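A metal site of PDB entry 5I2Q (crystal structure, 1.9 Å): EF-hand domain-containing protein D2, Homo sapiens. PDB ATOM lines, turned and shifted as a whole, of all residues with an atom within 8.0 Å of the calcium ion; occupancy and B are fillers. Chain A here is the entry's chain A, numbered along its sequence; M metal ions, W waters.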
ATOM      1  N   PHE A  37     -34.521  26.242 -22.005  1.00  0.00           N
ATOM      2  CA  PHE A  37     -33.334  25.468 -21.613  1.00  0.00           C
ATOM      3  C   PHE A  37     -32.446  26.286 -20.677  1.00  0.00           C
ATOM      4  O   PHE A  37     -32.063  25.815 -19.599  1.00  0.00           O
ATOM      5  CB  PHE A  37     -32.553  25.058 -22.862  1.00  0.00           C
ATOM      6  CG  PHE A  37     -31.392  24.139 -22.586  1.00  0.00           C
ATOM      7  CD1 PHE A  37     -31.587  22.760 -22.502  1.00  0.00           C
ATOM      8  CD2 PHE A  37     -30.102  24.645 -22.451  1.00  0.00           C
ATOM      9  CE1 PHE A  37     -30.509  21.912 -22.263  1.00  0.00           C
ATOM     10  CE2 PHE A  37     -29.016  23.790 -22.220  1.00  0.00           C
ATOM     11  CZ  PHE A  37     -29.220  22.428 -22.126  1.00  0.00           C
ATOM     12  N   TYR A  40     -33.582  26.826 -17.012  1.00  0.00           N
ATOM     13  CA  TYR A  40     -33.536  25.713 -16.073  1.00  0.00           C
ATOM     14  C   TYR A  40     -32.151  25.081 -15.888  1.00  0.00           C
ATOM     15  O   TYR A  40     -31.955  24.259 -14.997  1.00  0.00           O
ATOM     16  CB  TYR A  40     -34.574  24.656 -16.452  1.00  0.00           C
ATOM     17  CG  TYR A  40     -35.979  25.149 -16.210  1.00  0.00           C
ATOM     18  CD1 TYR A  40     -36.463  25.276 -14.928  1.00  0.00           C
ATOM     19  CD2 TYR A  40     -36.805  25.490 -17.275  1.00  0.00           C
ATOM     20  CE1 TYR A  40     -37.751  25.731 -14.692  1.00  0.00           C
ATOM     21  CE2 TYR A  40     -38.092  25.939 -17.055  1.00  0.00           C
ATOM     22  CZ  TYR A  40     -38.555  26.063 -15.752  1.00  0.00           C
ATOM     23  OH  TYR A  40     -39.836  26.508 -15.510  1.00  0.00           O
ATOM     24  N   ASP A  41     -31.201  25.498 -16.719  1.00  0.00           N
ATOM     25  CA  ASP A  41     -29.797  25.178 -16.494  1.00  0.00           C
ATOM     26  C   ASP A  41     -29.263  26.166 -15.463  1.00  0.00           C
ATOM     27  O   ASP A  41     -28.558  27.136 -15.803  1.00  0.00           O
ATOM     28  CB  ASP A  41     -28.994  25.284 -17.799  1.00  0.00           C
ATOM     29  CG  ASP A  41     -27.493  25.062 -17.604  1.00  0.00           C
ATOM     30  OD1 ASP A  41     -27.065  24.511 -16.563  1.00  0.00           O
ATOM     31  OD2 ASP A  41     -26.735  25.446 -18.529  1.00  0.00           O
ATOM     32  N   ALA A  42     -29.619  25.931 -14.201  1.00  0.00           N
ATOM     33  CA  ALA A  42     -29.247  26.818 -13.105  1.00  0.00           C
ATOM     34  C   ALA A  42     -27.731  26.893 -12.952  1.00  0.00           C
ATOM     35  O   ALA A  42     -27.196  27.926 -12.560  1.00  0.00           O
ATOM     36  CB  ALA A  42     -29.902  26.358 -11.797  1.00  0.00           C
ATOM     37  N   GLY A  43     -27.032  25.803 -13.291  1.00  0.00           N
ATOM     38  CA  GLY A  43     -25.595  25.756 -13.185  1.00  0.00           C
ATOM     39  C   GLY A  43     -24.798  26.446 -14.287  1.00  0.00           C
ATOM     40  O   GLY A  43     -23.583  26.636 -14.150  1.00  0.00           O
ATOM     41  N   ARG A  44     -25.469  26.807 -15.375  1.00  0.00           N
ATOM     42  CA  ARG A  44     -24.833  27.488 -16.517  1.00  0.00           C
ATOM     43  C   ARG A  44     -23.725  26.682 -17.199  1.00  0.00           C
ATOM     44  O   ARG A  44     -22.799  27.269 -17.765  1.00  0.00           O
ATOM     45  CB  ARG A  44     -24.261  28.859 -16.101  1.00  0.00           C
ATOM     46  CG  ARG A  44     -25.285  29.869 -15.579  1.00  0.00           C
ATOM     47  CD  ARG A  44     -24.670  31.268 -15.496  1.00  0.00           C
ATOM     48  NE  ARG A  44     -23.454  31.303 -14.676  1.00  0.00           N
ATOM     49  CZ  ARG A  44     -23.456  31.429 -13.346  1.00  0.00           C
ATOM     50  NH1 ARG A  44     -24.595  31.540 -12.687  1.00  0.00           N
ATOM     51  NH2 ARG A  44     -22.305  31.458 -12.687  1.00  0.00           N
ATOM     52  N   ASP A  45     -23.803  25.357 -17.168  1.00  0.00           N
ATOM     53  CA  ASP A  45     -22.760  24.539 -17.775  1.00  0.00           C
ATOM     54  C   ASP A  45     -23.134  24.061 -19.179  1.00  0.00           C
ATOM     55  O   ASP A  45     -22.334  23.430 -19.866  1.00  0.00           O
ATOM     56  CB  ASP A  45     -22.401  23.355 -16.882  1.00  0.00           C
ATOM     57  CG  ASP A  45     -23.537  22.349 -16.741  1.00  0.00           C
ATOM     58  OD1 ASP A  45     -24.720  22.733 -16.921  1.00  0.00           O
ATOM     59  OD2 ASP A  45     -23.253  21.169 -16.432  1.00  0.00           O
ATOM     60  N   GLY A  46     -24.364  24.346 -19.603  1.00  0.00           N
ATOM     61  CA  GLY A  46     -24.812  23.947 -20.927  1.00  0.00           C
ATOM     62  C   GLY A  46     -25.586  22.628 -20.931  1.00  0.00           C
ATOM     63  O   GLY A  46     -25.900  22.089 -21.993  1.00  0.00           O
ATOM     64  N   PHE A  47     -25.899  22.114 -19.739  1.00  0.00           N
ATOM     65  CA  PHE A  47     -26.670  20.872 -19.612  1.00  0.00           C
ATOM     66  C   PHE A  47     -27.797  21.046 -18.594  1.00  0.00           C
ATOM     67  O   PHE A  47     -27.690  21.847 -17.669  1.00  0.00           O
ATOM     68  CB  PHE A  47     -25.780  19.695 -19.152  1.00  0.00           C
ATOM     69  CG  PHE A  47     -24.686  19.345 -20.126  1.00  0.00           C
ATOM     70  CD1 PHE A  47     -24.924  18.451 -21.171  1.00  0.00           C
ATOM     71  CD2 PHE A  47     -23.415  19.901 -19.995  1.00  0.00           C
ATOM     72  CE1 PHE A  47     -23.919  18.121 -22.085  1.00  0.00           C
ATOM     73  CE2 PHE A  47     -22.397  19.569 -20.894  1.00  0.00           C
ATOM     74  CZ  PHE A  47     -22.656  18.685 -21.945  1.00  0.00           C
ATOM     75  N   ILE A  48     -28.862  20.283 -18.764  1.00  0.00           N
ATOM     76  CA  ILE A  48     -29.837  20.113 -17.690  1.00  0.00           C
ATOM     77  C   ILE A  48     -29.632  18.709 -17.116  1.00  0.00           C
ATOM     78  O   ILE A  48     -29.883  17.701 -17.795  1.00  0.00           O
ATOM     79  CB  ILE A  48     -31.280  20.343 -18.207  1.00  0.00           C
ATOM     80  CG1 ILE A  48     -31.482  21.839 -18.466  1.00  0.00           C
ATOM     81  CG2 ILE A  48     -32.319  19.832 -17.202  1.00  0.00           C
ATOM     82  CD1 ILE A  48     -32.829  22.202 -19.035  1.00  0.00           C
ATOM     83  N   ASP A  49     -29.144  18.648 -15.876  1.00  0.00           N
ATOM     84  CA  ASP A  49     -28.894  17.348 -15.238  1.00  0.00           C
ATOM     85  C   ASP A  49     -30.123  16.884 -14.464  1.00  0.00           C
ATOM     86  O   ASP A  49     -31.163  17.565 -14.461  1.00  0.00           O
ATOM     87  CB  ASP A  49     -27.636  17.361 -14.336  1.00  0.00           C
ATOM     88  CG  ASP A  49     -27.711  18.363 -13.171  1.00  0.00           C
ATOM     89  OD1 ASP A  49     -28.818  18.609 -12.614  1.00  0.00           O
ATOM     90  OD2 ASP A  49     -26.646  18.918 -12.783  1.00  0.00           O
ATOM     91  N   LEU A  50     -30.009  15.730 -13.805  1.00  0.00           N
ATOM     92  CA  LEU A  50     -31.156  15.121 -13.138  1.00  0.00           C
ATOM     93  C   LEU A  50     -31.761  16.045 -12.066  1.00  0.00           C
ATOM     94  O   LEU A  50     -32.968  16.142 -11.944  1.00  0.00           O
ATOM     95  CB  LEU A  50     -30.760  13.777 -12.507  1.00  0.00           C
ATOM     96  CG  LEU A  50     -31.899  13.063 -11.774  1.00  0.00           C
ATOM     97  CD1 LEU A  50     -32.624  12.112 -12.728  1.00  0.00           C
ATOM     98  CD2 LEU A  50     -31.376  12.297 -10.580  1.00  0.00           C
ATOM     99  N   GLU A  52     -31.530  19.380 -11.869  1.00  0.00           N
ATOM    100  CA  GLU A  52     -32.136  20.544 -12.523  1.00  0.00           C
ATOM    101  C   GLU A  52     -33.453  20.184 -13.206  1.00  0.00           C
ATOM    102  O   GLU A  52     -34.404  20.975 -13.196  1.00  0.00           O
ATOM    103  CB  GLU A  52     -31.169  21.141 -13.533  1.00  0.00           C
ATOM    104  CG  GLU A  52     -29.951  21.793 -12.879  1.00  0.00           C
ATOM    105  CD  GLU A  52     -28.831  22.054 -13.876  1.00  0.00           C
ATOM    106  OE1 GLU A  52     -28.659  21.220 -14.797  1.00  0.00           O
ATOM    107  OE2 GLU A  52     -28.133  23.094 -13.741  1.00  0.00           O
ATOM    108  N   LEU A  53     -33.456  19.001 -13.752  1.00  0.00           N
ATOM    109  CA  LEU A  53     -34.712  18.587 -14.388  1.00  0.00           C
ATOM    110  C   LEU A  53     -35.786  18.277 -13.329  1.00  0.00           C
ATOM    111  O   LEU A  53     -36.975  18.570 -13.513  1.00  0.00           O
ATOM    112  CB  LEU A  53     -34.487  17.346 -15.246  1.00  0.00           C
ATOM    113  CG  LEU A  53     -35.627  16.646 -15.981  1.00  0.00           C
ATOM    114  CD1 LEU A  53     -36.268  17.566 -17.030  1.00  0.00           C
ATOM    115  CD2 LEU A  53     -35.264  15.280 -16.552  1.00  0.00           C
ATOM    116  N   LYS A  83     -27.006  13.487 -19.023  1.00  0.00           N
ATOM    117  CA  LYS A  83     -27.791  14.682 -18.742  1.00  0.00           C
ATOM    118  C   LYS A  83     -28.218  15.243 -20.092  1.00  0.00           C
ATOM    119  O   LYS A  83     -27.809  14.713 -21.130  1.00  0.00           O
ATOM    120  CB  LYS A  83     -26.947  15.700 -17.955  1.00  0.00           C
ATOM    121  CG  LYS A  83     -25.516  15.821 -18.442  1.00  0.00           C
ATOM    122  CD  LYS A  83     -24.700  16.628 -17.437  1.00  0.00           C
ATOM    123  CE  LYS A  83     -23.277  16.831 -17.923  1.00  0.00           C
ATOM    124  NZ  LYS A  83     -22.598  15.534 -18.109  1.00  0.00           N
ATOM    125  N   LEU A  84     -29.045  16.286 -20.095  1.00  0.00           N
ATOM    126  CA  LEU A  84     -29.592  16.815 -21.343  1.00  0.00           C
ATOM    127  C   LEU A  84     -28.736  17.966 -21.898  1.00  0.00           C
ATOM    128  O   LEU A  84     -28.673  19.041 -21.294  1.00  0.00           O
ATOM    129  CB  LEU A  84     -30.996  17.359 -21.098  1.00  0.00           C
ATOM    130  CG  LEU A  84     -32.050  16.412 -20.540  1.00  0.00           C
ATOM    131  CD1 LEU A  84     -33.330  17.206 -20.251  1.00  0.00           C
ATOM    132  CD2 LEU A  84     -32.319  15.328 -21.573  1.00  0.00           C
HETATM  133 CA    CA M   1     -26.661  22.424 -15.647  1.00  0.00          CA
HETATM  134  O   HOH W   1     -25.577  20.121 -15.402  1.00  0.00           O
HETATM  135  O   HOH W   2     -24.911  22.553 -13.729  1.00  0.00           O
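The side-chain carboxylate (OD1) of Asp 41 lies close to the backbone NH (N) of Arg 44, 3.0 Å away. N of Gly 46 lies within hydrogen-bond range of OD2 of Asp 41 (2.8 Å). The side-chain carboxylate (OE2) of Glu 52 lies close to the backbone NH (N) of Gly 43 (3.0 Å). N of Glu 52 sits at hydrogen-bond distance from OD1 of Asp 49, 2.9 Å away. N of Ala 42 sits close to OE2 of Glu 52 (3.2 Å).
Four residues have an atom within 4 Å of the calcium ion: Asp 41, Asp 45, Phe 47 and Glu 52. Along chain A the residues within 4 Å of the calcium ion span positions 41 to 52.
The side-chain carboxylate (OD1) of Asp 41 binds the calcium ion (2.3 Å). The calcium ion is bound by O of Phe 47, 2.3 Å away. OD1 of Asp 45 binds the calcium ion, at 2.3 Å. The calcium ion is bound by the side-chain carboxylate (OE1) of Glu 52. The calcium ion is bound by OE2 of Glu 52 (2.5 Å). Water W1 binds the calcium ion. Water W2 is bound to the calcium ion (2.6 Å). The calcium ion has seven donor atoms within binding distance.
Water W1 lies within hydrogen-bond range of the side-chain carboxylate (OD2) of Asp 45 (2.7 Å) and the side-chain carboxylate (OD2) of Asp 49 (3.1 Å).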
